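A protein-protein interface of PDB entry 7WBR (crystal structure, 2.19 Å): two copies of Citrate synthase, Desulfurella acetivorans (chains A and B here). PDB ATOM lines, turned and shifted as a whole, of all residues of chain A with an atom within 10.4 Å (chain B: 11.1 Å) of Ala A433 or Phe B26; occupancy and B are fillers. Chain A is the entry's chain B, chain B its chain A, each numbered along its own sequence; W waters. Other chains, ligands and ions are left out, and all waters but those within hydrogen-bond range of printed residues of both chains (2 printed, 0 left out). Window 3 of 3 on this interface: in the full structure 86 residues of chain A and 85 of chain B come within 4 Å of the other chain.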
ATOM      1  N   VAL A  34       3.130   9.235  -6.177  1.00  0.00           N
ATOM      2  CA  VAL A  34       3.407   7.835  -5.833  1.00  0.00           C
ATOM      3  C   VAL A  34       4.910   7.686  -5.596  1.00  0.00           C
ATOM      4  O   VAL A  34       5.727   8.114  -6.420  1.00  0.00           O
ATOM      5  CB  VAL A  34       2.942   6.856  -6.942  1.00  0.00           C
ATOM      6  CG1 VAL A  34       3.165   5.412  -6.525  1.00  0.00           C
ATOM      7  CG2 VAL A  34       1.483   7.097  -7.310  1.00  0.00           C
ATOM      8  N   THR A  35       5.286   7.116  -4.464  1.00  0.00           N
ATOM      9  CA  THR A  35       6.702   6.866  -4.192  1.00  0.00           C
ATOM     10  C   THR A  35       6.991   5.375  -4.308  1.00  0.00           C
ATOM     11  O   THR A  35       6.068   4.570  -4.339  1.00  0.00           O
ATOM     12  CB  THR A  35       7.104   7.401  -2.804  1.00  0.00           C
ATOM     13  OG1 THR A  35       6.602   6.548  -1.746  1.00  0.00           O
ATOM     14  CG2 THR A  35       6.622   8.920  -2.646  1.00  0.00           C
ATOM     15  N   ILE A  36       8.263   5.025  -4.371  1.00  0.00           N
ATOM     16  CA  ILE A  36       8.714   3.636  -4.340  1.00  0.00           C
ATOM     17  C   ILE A  36       8.146   2.883  -3.124  1.00  0.00           C
ATOM     18  O   ILE A  36       7.788   1.704  -3.228  1.00  0.00           O
ATOM     19  CB  ILE A  36      10.267   3.574  -4.306  1.00  0.00           C
ATOM     20  CG1 ILE A  36      10.802   4.022  -5.663  1.00  0.00           C
ATOM     21  CG2 ILE A  36      10.780   2.204  -3.889  1.00  0.00           C
ATOM     22  CD1 ILE A  36      12.274   3.839  -5.872  1.00  0.00           C
ATOM     23  N   SER A  37       8.172   3.565  -1.981  1.00  0.00           N
ATOM     24  CA  SER A  37       7.662   3.093  -0.673  1.00  0.00           C
ATOM     25  C   SER A  37       6.192   2.720  -0.705  1.00  0.00           C
ATOM     26  O   SER A  37       5.795   1.746  -0.065  1.00  0.00           O
ATOM     27  CB  SER A  37       7.795   4.176   0.404  1.00  0.00           C
ATOM     28  OG  SER A  37       7.748   3.577   1.691  1.00  0.00           O
ATOM     29  N   GLN A  38       5.421   3.557  -1.389  1.00  0.00           N
ATOM     30  CA  GLN A  38       3.980   3.390  -1.561  1.00  0.00           C
ATOM     31  C   GLN A  38       3.602   2.329  -2.607  1.00  0.00           C
ATOM     32  O   GLN A  38       2.600   1.626  -2.452  1.00  0.00           O
ATOM     33  CB  GLN A  38       3.360   4.725  -1.979  1.00  0.00           C
ATOM     34  CG  GLN A  38       3.490   5.814  -0.928  1.00  0.00           C
ATOM     35  CD  GLN A  38       2.896   7.112  -1.420  1.00  0.00           C
ATOM     36  OE1 GLN A  38       3.320   7.626  -2.438  1.00  0.00           O
ATOM     37  NE2 GLN A  38       1.850   7.615  -0.734  1.00  0.00           N
ATOM     38  N   ALA A  39       4.398   2.180  -3.663  1.00  0.00           N
ATOM     39  CA  ALA A  39       4.181   1.050  -4.626  1.00  0.00           C
ATOM     40  C   ALA A  39       4.442  -0.311  -3.965  1.00  0.00           C
ATOM     41  O   ALA A  39       3.665  -1.266  -4.083  1.00  0.00           O
ATOM     42  CB  ALA A  39       5.074   1.218  -5.843  1.00  0.00           C
ATOM     43  N   ILE A  40       5.544  -0.392  -3.241  1.00  0.00           N
ATOM     44  CA  ILE A  40       5.858  -1.558  -2.467  1.00  0.00           C
ATOM     45  C   ILE A  40       4.954  -1.693  -1.258  1.00  0.00           C
ATOM     46  O   ILE A  40       4.721  -2.795  -0.818  1.00  0.00           O
ATOM     47  CB  ILE A  40       7.332  -1.514  -2.023  1.00  0.00           C
ATOM     48  CG1 ILE A  40       8.243  -1.657  -3.268  1.00  0.00           C
ATOM     49  CG2 ILE A  40       7.642  -2.571  -0.976  1.00  0.00           C
ATOM     50  CD1 ILE A  40       9.719  -1.468  -2.952  1.00  0.00           C
ATOM     51  N   ARG A  44      -0.116   2.656   0.235  1.00  0.00           N
ATOM     52  CA  ARG A  44      -0.429   3.382   1.495  1.00  0.00           C
ATOM     53  C   ARG A  44      -0.477   4.900   1.260  1.00  0.00           C
ATOM     54  O   ARG A  44       0.427   5.431   0.642  1.00  0.00           O
ATOM     55  CB  ARG A  44       0.640   3.012   2.526  1.00  0.00           C
ATOM     56  CG  ARG A  44       0.489   3.538   3.954  1.00  0.00           C
ATOM     57  CD  ARG A  44       1.773   3.275   4.782  1.00  0.00           C
ATOM     58  NE  ARG A  44       3.020   3.628   4.041  1.00  0.00           N
ATOM     59  CZ  ARG A  44       4.017   2.801   3.658  1.00  0.00           C
ATOM     60  NH1 ARG A  44       5.044   3.315   2.961  1.00  0.00           N
ATOM     61  NH2 ARG A  44       4.028   1.485   3.946  1.00  0.00           N
ATOM     62  N   THR A 426      10.831  -4.678  -9.836  1.00  0.00           N
ATOM     63  CA  THR A 426      11.844  -4.203  -8.914  1.00  0.00           C
ATOM     64  C   THR A 426      13.083  -3.703  -9.709  1.00  0.00           C
ATOM     65  O   THR A 426      13.667  -2.741  -9.294  1.00  0.00           O
ATOM     66  CB  THR A 426      12.024  -5.029  -7.581  1.00  0.00           C
ATOM     67  OG1 THR A 426      13.402  -5.286  -7.214  1.00  0.00           O
ATOM     68  CG2 THR A 426      11.348  -6.197  -7.618  1.00  0.00           C
ATOM     69  N   ASP A 427      13.367  -4.240 -10.895  1.00  0.00           N
ATOM     70  CA  ASP A 427      14.376  -3.651 -11.783  1.00  0.00           C
ATOM     71  C   ASP A 427      13.978  -2.205 -12.127  1.00  0.00           C
ATOM     72  O   ASP A 427      14.804  -1.332 -12.164  1.00  0.00           O
ATOM     73  CB  ASP A 427      14.563  -4.399 -13.129  1.00  0.00           C
ATOM     74  CG  ASP A 427      15.209  -5.760 -12.995  1.00  0.00           C
ATOM     75  OD1 ASP A 427      15.798  -6.092 -11.956  1.00  0.00           O
ATOM     76  OD2 ASP A 427      15.114  -6.533 -13.979  1.00  0.00           O
ATOM     77  N   MET A 428      12.725  -1.967 -12.443  1.00  0.00           N
ATOM     78  CA  MET A 428      12.297  -0.603 -12.750  1.00  0.00           C
ATOM     79  C   MET A 428      12.360   0.351 -11.564  1.00  0.00           C
ATOM     80  O   MET A 428      12.647   1.519 -11.756  1.00  0.00           O
ATOM     81  CB  MET A 428      10.914  -0.592 -13.329  1.00  0.00           C
ATOM     82  CG  MET A 428      10.890  -1.148 -14.741  1.00  0.00           C
ATOM     83  SD  MET A 428       9.188  -1.498 -15.158  1.00  0.00           S
ATOM     84  CE  MET A 428       8.513   0.138 -15.519  1.00  0.00           C
ATOM     85  N   LEU A 429      12.102  -0.152 -10.360  1.00  0.00           N
ATOM     86  CA  LEU A 429      12.231   0.662  -9.151  1.00  0.00           C
ATOM     87  C   LEU A 429      13.695   0.974  -8.790  1.00  0.00           C
ATOM     88  O   LEU A 429      13.980   2.044  -8.265  1.00  0.00           O
ATOM     89  CB  LEU A 429      11.593  -0.015  -7.948  1.00  0.00           C
ATOM     90  CG  LEU A 429      10.070  -0.222  -7.951  1.00  0.00           C
ATOM     91  CD1 LEU A 429       9.694  -1.221  -6.847  1.00  0.00           C
ATOM     92  CD2 LEU A 429       9.274   1.063  -7.827  1.00  0.00           C
ATOM     93  N   GLU A 430      14.560  -0.018  -8.972  1.00  0.00           N
ATOM     94  CA  GLU A 430      15.984   0.136  -8.869  1.00  0.00           C
ATOM     95  C   GLU A 430      16.493   1.153  -9.884  1.00  0.00           C
ATOM     96  O   GLU A 430      17.361   1.955  -9.541  1.00  0.00           O
ATOM     97  CB  GLU A 430      16.710  -1.213  -8.990  1.00  0.00           C
ATOM     98  CG  GLU A 430      16.593  -2.020  -7.712  1.00  0.00           C
ATOM     99  CD  GLU A 430      17.119  -3.423  -7.796  1.00  0.00           C
ATOM    100  OE1 GLU A 430      17.388  -3.857  -8.920  1.00  0.00           O
ATOM    101  OE2 GLU A 430      17.265  -4.092  -6.738  1.00  0.00           O
ATOM    102  N   LYS A 431      15.943   1.180 -11.087  1.00  0.00           N
ATOM    103  CA  LYS A 431      16.345   2.226 -12.060  1.00  0.00           C
ATOM    104  C   LYS A 431      16.068   3.635 -11.556  1.00  0.00           C
ATOM    105  O   LYS A 431      16.900   4.527 -11.734  1.00  0.00           O
ATOM    106  CB  LYS A 431      15.702   2.052 -13.433  1.00  0.00           C
ATOM    107  CG  LYS A 431      16.412   1.062 -14.340  1.00  0.00           C
ATOM    108  CD  LYS A 431      15.786   1.073 -15.744  1.00  0.00           C
ATOM    109  CE  LYS A 431      16.449   0.069 -16.701  1.00  0.00           C
ATOM    110  NZ  LYS A 431      16.560  -1.309 -16.116  1.00  0.00           N
ATOM    111  N   TRP A 432      14.913   3.838 -10.925  1.00  0.00           N
ATOM    112  CA  TRP A 432      14.683   5.055 -10.156  1.00  0.00           C
ATOM    113  C   TRP A 432      15.787   5.055  -9.000  1.00  0.00           C
ATOM    114  O   TRP A 432      15.601   4.575  -7.886  1.00  0.00           O
ATOM    115  CB  TRP A 432      13.161   5.127  -9.772  1.00  0.00           C
ATOM    116  CG  TRP A 432      12.131   5.546 -10.956  1.00  0.00           C
ATOM    117  CD1 TRP A 432      12.050   6.793 -11.589  1.00  0.00           C
ATOM    118  CD2 TRP A 432      11.023   4.762 -11.542  1.00  0.00           C
ATOM    119  NE1 TRP A 432      11.009   6.811 -12.511  1.00  0.00           N
ATOM    120  CE2 TRP A 432      10.373   5.599 -12.514  1.00  0.00           C
ATOM    121  CE3 TRP A 432      10.524   3.460 -11.339  1.00  0.00           C
ATOM    122  CZ2 TRP A 432       9.269   5.151 -13.294  1.00  0.00           C
ATOM    123  CZ3 TRP A 432       9.424   3.011 -12.118  1.00  0.00           C
ATOM    124  CH2 TRP A 432       8.824   3.854 -13.089  1.00  0.00           C
ATOM    125  N   ALA A 433      17.005   5.497  -9.384  1.00  0.00           N
ATOM    126  CA  ALA A 433      18.337   5.319  -8.672  1.00  0.00           C
ATOM    127  C   ALA A 433      19.209   4.141  -9.118  1.00  0.00           C
ATOM    128  O   ALA A 433      20.445   4.117  -8.942  1.00  0.00           O
ATOM    129  CB  ALA A 433      18.205   5.316  -7.161  1.00  0.00           C
ATOM    130  N   PRO B  17      16.840  -8.711  -0.167  1.00  0.00           N
ATOM    131  CA  PRO B  17      17.673  -7.514   0.131  1.00  0.00           C
ATOM    132  C   PRO B  17      17.426  -6.356  -0.810  1.00  0.00           C
ATOM    133  O   PRO B  17      17.500  -5.202  -0.406  1.00  0.00           O
ATOM    134  CB  PRO B  17      19.106  -8.033  -0.021  1.00  0.00           C
ATOM    135  CG  PRO B  17      19.001  -9.503   0.245  1.00  0.00           C
ATOM    136  CD  PRO B  17      17.671  -9.920  -0.320  1.00  0.00           C
ATOM    137  N   ARG B  18      17.111  -6.676  -2.056  1.00  0.00           N
ATOM    138  CA  ARG B  18      16.783  -5.667  -3.041  1.00  0.00           C
ATOM    139  C   ARG B  18      15.578  -4.821  -2.629  1.00  0.00           C
ATOM    140  O   ARG B  18      15.602  -3.599  -2.802  1.00  0.00           O
ATOM    141  CB  ARG B  18      16.523  -6.298  -4.399  1.00  0.00           C
ATOM    142  CG  ARG B  18      17.759  -7.024  -4.954  1.00  0.00           C
ATOM    143  CD  ARG B  18      17.433  -7.880  -6.161  1.00  0.00           C
ATOM    144  NE  ARG B  18      17.078  -7.066  -7.298  1.00  0.00           N
ATOM    145  CZ  ARG B  18      16.282  -7.439  -8.295  1.00  0.00           C
ATOM    146  NH1 ARG B  18      15.663  -8.609  -8.285  1.00  0.00           N
ATOM    147  NH2 ARG B  18      16.045  -6.607  -9.293  1.00  0.00           N
ATOM    148  N   THR B  19      14.540  -5.492  -2.108  1.00  0.00           N
ATOM    149  CA  THR B  19      13.314  -4.841  -1.621  1.00  0.00           C
ATOM    150  C   THR B  19      13.645  -4.065  -0.321  1.00  0.00           C
ATOM    151  O   THR B  19      13.170  -2.959  -0.112  1.00  0.00           O
ATOM    152  CB  THR B  19      12.106  -5.846  -1.381  1.00  0.00           C
ATOM    153  OG1 THR B  19      11.814  -6.586  -2.571  1.00  0.00           O
ATOM    154  CG2 THR B  19      10.842  -5.101  -0.995  1.00  0.00           C
ATOM    155  N   THR B  20      14.424  -4.670   0.552  1.00  0.00           N
ATOM    156  CA  THR B  20      14.811  -4.014   1.795  1.00  0.00           C
ATOM    157  C   THR B  20      15.567  -2.710   1.499  1.00  0.00           C
ATOM    158  O   THR B  20      15.232  -1.663   2.029  1.00  0.00           O
ATOM    159  CB  THR B  20      15.669  -4.955   2.627  1.00  0.00           C
ATOM    160  OG1 THR B  20      15.025  -6.224   2.642  1.00  0.00           O
ATOM    161  CG2 THR B  20      15.850  -4.453   4.051  1.00  0.00           C
ATOM    162  N   ARG B  21      16.512  -2.776   0.571  1.00  0.00           N
ATOM    163  CA  ARG B  21      17.289  -1.633   0.189  1.00  0.00           C
ATOM    164  C   ARG B  21      16.493  -0.489  -0.404  1.00  0.00           C
ATOM    165  O   ARG B  21      16.727   0.677  -0.049  1.00  0.00           O
ATOM    166  CB  ARG B  21      18.375  -2.028  -0.804  1.00  0.00           C
ATOM    167  CG  ARG B  21      19.375  -0.895  -1.016  1.00  0.00           C
ATOM    168  CD  ARG B  21      20.804  -1.378  -0.951  1.00  0.00           C
ATOM    169  NE  ARG B  21      21.385  -1.506  -2.269  1.00  0.00           N
ATOM    170  CZ  ARG B  21      21.826  -0.495  -3.006  1.00  0.00           C
ATOM    171  NH1 ARG B  21      21.718   0.765  -2.587  1.00  0.00           N
ATOM    172  NH2 ARG B  21      22.364  -0.757  -4.195  1.00  0.00           N
ATOM    173  N   LEU B  22      15.595  -0.759  -1.342  1.00  0.00           N
ATOM    174  CA  LEU B  22      14.870   0.394  -1.871  1.00  0.00           C
ATOM    175  C   LEU B  22      13.831   0.955  -0.860  1.00  0.00           C
ATOM    176  O   LEU B  22      13.419   2.081  -0.994  1.00  0.00           O
ATOM    177  CB  LEU B  22      14.429   0.266  -3.352  1.00  0.00           C
ATOM    178  CG  LEU B  22      13.531  -0.756  -4.023  1.00  0.00           C
ATOM    179  CD1 LEU B  22      14.225  -1.564  -5.102  1.00  0.00           C
ATOM    180  CD2 LEU B  22      12.890  -1.647  -2.981  1.00  0.00           C
ATOM    181  N   LEU B  23      13.485   0.197   0.169  1.00  0.00           N
ATOM    182  CA  LEU B  23      12.658   0.693   1.264  1.00  0.00           C
ATOM    183  C   LEU B  23      13.494   1.467   2.301  1.00  0.00           C
ATOM    184  O   LEU B  23      13.042   2.485   2.800  1.00  0.00           O
ATOM    185  CB  LEU B  23      11.893  -0.471   1.955  1.00  0.00           C
ATOM    186  CG  LEU B  23      10.359  -0.507   1.909  1.00  0.00           C
ATOM    187  CD1 LEU B  23       9.829  -0.124   0.529  1.00  0.00           C
ATOM    188  CD2 LEU B  23       9.830  -1.878   2.381  1.00  0.00           C
ATOM    189  N   LYS B  24      14.673   0.930   2.654  1.00  0.00           N
ATOM    190  CA  LYS B  24      15.597   1.572   3.605  1.00  0.00           C
ATOM    191  C   LYS B  24      16.082   2.907   3.042  1.00  0.00           C
ATOM    192  O   LYS B  24      15.917   3.923   3.707  1.00  0.00           O
ATOM    193  CB  LYS B  24      16.811   0.675   3.932  1.00  0.00           C
ATOM    194  N   GLU B  25      16.593   2.894   1.796  1.00  0.00           N
ATOM    195  CA  GLU B  25      17.326   4.028   1.226  1.00  0.00           C
ATOM    196  C   GLU B  25      16.615   4.887   0.213  1.00  0.00           C
ATOM    197  O   GLU B  25      16.917   6.062   0.162  1.00  0.00           O
ATOM    198  CB  GLU B  25      18.616   3.555   0.563  1.00  0.00           C
ATOM    199  CG  GLU B  25      19.631   2.947   1.516  1.00  0.00           C
ATOM    200  CD  GLU B  25      20.813   2.339   0.760  1.00  0.00           C
ATOM    201  OE1 GLU B  25      21.239   2.962  -0.244  1.00  0.00           O
ATOM    202  OE2 GLU B  25      21.295   1.240   1.154  1.00  0.00           O
ATOM    203  N   PHE B  26      15.707   4.331  -0.608  1.00  0.00           N
ATOM    204  CA  PHE B  26      15.047   5.108  -1.687  1.00  0.00           C
ATOM    205  C   PHE B  26      13.502   5.229  -1.561  1.00  0.00           C
ATOM    206  O   PHE B  26      12.799   5.532  -2.522  1.00  0.00           O
ATOM    207  CB  PHE B  26      15.515   4.604  -3.070  1.00  0.00           C
ATOM    208  CG  PHE B  26      17.020   4.528  -3.195  1.00  0.00           C
ATOM    209  CD1 PHE B  26      17.768   5.680  -3.464  1.00  0.00           C
ATOM    210  CD2 PHE B  26      17.701   3.342  -2.922  1.00  0.00           C
ATOM    211  CE1 PHE B  26      19.161   5.636  -3.513  1.00  0.00           C
ATOM    212  CE2 PHE B  26      19.098   3.288  -2.994  1.00  0.00           C
ATOM    213  CZ  PHE B  26      19.828   4.443  -3.295  1.00  0.00           C
ATOM    214  N   GLY B  27      13.009   5.089  -0.342  1.00  0.00           N
ATOM    215  CA  GLY B  27      11.555   5.053  -0.077  1.00  0.00           C
ATOM    216  C   GLY B  27      10.803   6.202  -0.689  1.00  0.00           C
ATOM    217  O   GLY B  27       9.691   6.019  -1.204  1.00  0.00           O
ATOM    218  N   ASN B  28      11.430   7.386  -0.712  1.00  0.00           N
ATOM    219  CA  ASN B  28      10.755   8.603  -1.208  1.00  0.00           C
ATOM    220  C   ASN B  28      10.968   8.966  -2.647  1.00  0.00           C
ATOM    221  O   ASN B  28      10.472   9.982  -3.073  1.00  0.00           O
ATOM    222  CB  ASN B  28      11.120   9.783  -0.325  1.00  0.00           C
ATOM    223  CG  ASN B  28      10.547   9.631   1.051  1.00  0.00           C
ATOM    224  OD1 ASN B  28      11.245   9.238   1.983  1.00  0.00           O
ATOM    225  ND2 ASN B  28       9.243   9.883   1.182  1.00  0.00           N
ATOM    226  N   VAL B  29      11.677   8.155  -3.422  1.00  0.00           N
ATOM    227  CA  VAL B  29      11.867   8.521  -4.833  1.00  0.00           C
ATOM    228  C   VAL B  29      10.498   8.472  -5.489  1.00  0.00           C
ATOM    229  O   VAL B  29       9.786   7.496  -5.334  1.00  0.00           O
ATOM    230  CB  VAL B  29      12.855   7.591  -5.556  1.00  0.00           C
ATOM    231  CG1 VAL B  29      12.863   7.838  -7.055  1.00  0.00           C
ATOM    232  CG2 VAL B  29      14.253   7.763  -4.975  1.00  0.00           C
ATOM    233  N   LYS B  30      10.158   9.555  -6.171  1.00  0.00           N
ATOM    234  CA  LYS B  30       8.950   9.689  -6.964  1.00  0.00           C
ATOM    235  C   LYS B  30       8.970   8.903  -8.295  1.00  0.00           C
ATOM    236  O   LYS B  30       9.957   8.942  -9.075  1.00  0.00           O
ATOM    237  CB  LYS B  30       8.675  11.155  -7.257  1.00  0.00           C
ATOM    238  CG  LYS B  30       7.468  11.368  -8.144  1.00  0.00           C
ATOM    239  CD  LYS B  30       6.924  12.789  -8.066  1.00  0.00           C
ATOM    240  CE  LYS B  30       6.397  13.186  -9.439  1.00  0.00           C
ATOM    241  NZ  LYS B  30       5.503  14.345  -9.315  1.00  0.00           N
ATOM    242  N   ILE B  31       7.828   8.249  -8.541  1.00  0.00           N
ATOM    243  CA  ILE B  31       7.620   7.279  -9.576  1.00  0.00           C
ATOM    244  C   ILE B  31       6.488   7.677 -10.517  1.00  0.00           C
ATOM    245  O   ILE B  31       6.485   7.321 -11.702  1.00  0.00           O
ATOM    246  CB  ILE B  31       7.357   5.917  -8.871  1.00  0.00           C
ATOM    247  CG1 ILE B  31       8.325   4.891  -9.380  1.00  0.00           C
ATOM    248  CG2 ILE B  31       5.910   5.408  -8.919  1.00  0.00           C
ATOM    249  CD1 ILE B  31       9.624   5.060  -8.648  1.00  0.00           C
ATOM    250  N   ASP B  32       5.487   8.385 -10.001  1.00  0.00           N
ATOM    251  CA  ASP B  32       4.420   8.833 -10.847  1.00  0.00           C
ATOM    252  C   ASP B  32       3.607   9.918 -10.158  1.00  0.00           C
ATOM    253  O   ASP B  32       3.786  10.190  -8.980  1.00  0.00           O
ATOM    254  CB  ASP B  32       3.498   7.645 -11.153  1.00  0.00           C
ATOM    255  CG  ASP B  32       2.787   7.794 -12.434  1.00  0.00           C
ATOM    256  OD1 ASP B  32       2.849   8.891 -13.061  1.00  0.00           O
ATOM    257  OD2 ASP B  32       2.151   6.810 -12.827  1.00  0.00           O
HETATM  258  O   HOH W   1      17.523  -2.903  -4.291  1.00  0.00           O
HETATM  259  O   HOH W   2      17.808  -7.651 -11.992  1.00  0.00           O
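The backbone carbonyl oxygen of Gly B27 sits at hydrogen-bond distance from the side-chain hydroxyl of Thr A35, 3.2 Å away.
O of Val A34 is in hydrogen-bond range of N of Ile B31.
The backbone carbonyl oxygen (O) of Val B29 lies within hydrogen-bond range of the backbone NH (N) of Ile A36, 3.1 Å away.
The guanidinium group of Arg B18 lies within salt-bridge range of the side-chain carboxylate of Asp A427, at 2.7 Å.
O of Gly B27 is in hydrogen-bond range of N of Ser A37 (3.0 Å).
The backbone carbonyl oxygen (O) of Asp B32 sits at hydrogen-bond distance from the backbone NH (N) of Val A34, at 3.0 Å.
NE of Arg B18 is in salt-bridge range of OE2 of Glu A430 (3.0 Å).
The backbone NH (N) of Thr A35 sits at hydrogen-bond distance from the side-chain amide oxygen (OE1) of Gln A38, at 2.9 Å.
OG1 of Thr A35 sits close to N of Ser A37, 3.4 Å away.
O of Leu B22 sits at hydrogen-bond distance from N of Gly B27.
The side-chain hydroxyl (OG) of Ser A37 lies within hydrogen-bond range of the guanidinium group (NH1) of Arg A44.
Val A34 touches Lys B30.
Thr A35 touches Val B29.
Ile A36 touches Gly B27 (N to O, 3.6 Å).
Ile A36 touches Ile B31.
CD1 of Ile A40 touches CD2 of Leu B22, 3.2 Å away.
CD1 of Leu B23 touches CG2 of Ile A40, at 3.6 Å.
Leu B22 touches Glu A430.
CG1 of Val B29 touches CB of Trp A432, at 3.8 Å.
Trp A432 touches Lys B30 (CD1 to O, 3.9 Å).
Ile B31 touches Trp A432.
Of chain B, only Leu B22 (3.9 Å), Phe B26 (3.7 Å), Gly B27 (3.6 Å), Val B29 (3.1 Å) and Ile B31 (3.4 Å) come within 4 Å of Ile A36.
Of the printed residues of chain B, Glu A430 touches Arg B18 and Leu B22.
Printed residues of chain B within 4 Å of Trp A432: Val B29 (3.8 Å), Lys B30 (3.9 Å) and Ile B31 (3.2 Å).
Of the printed residues of chain B, Ala A433 touches Phe B26.
Thr B19 touches none of the printed residues of chain A.
No residue of chain A comes within 4 Å of Lys B24.
Glu B25 touches none of the printed residues of chain A.
Of chain A, only Ile A36 and Ala A433 come within 4 Å of Phe B26.
Asn B28 touches none of the printed residues of chain A.
Of chain A, only Thr A35, Ile A36 and Trp A432 come within 4 Å of Val B29.
The nearest residue of chain A that does not touch Phe B26 is Trp A432 (4.8 Å).
Of the 16 printed residues of chain A, 10 touch a printed residue of chain B.
Hydrophobic or aromatic side chains of chain A that line the printed part of chain B: Val A34, Ile A36, Ile A40, Trp A432 and Ala A433.
Along chain A the printed residues that touch a printed residue of chain B span positions 34 to 433.
Of the 16 printed residues of chain B, 9 touch a printed residue of chain A.
Among the printed residues, 21 pairs touch across the chains.
Among the printed residues, Asp or Glu carboxylates within 4 Å of a Lys or Arg side-chain nitrogen of the other chain: Asp A427 with Arg B18 (2.7 Å) and Glu A430 with Arg B18 (3.0 Å).
No position is printed for both chains.
Water W1 bridges the backbone carbonyl oxygen (O) of Arg B18 (2.5 Å) and the side-chain carboxylate (OE2) of Glu A430 (2.7 Å).
Water W2 lies within hydrogen-bond range of OD1 of Asp A427 (2.5 Å) and NH2 of Arg B18 (3.4 Å).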
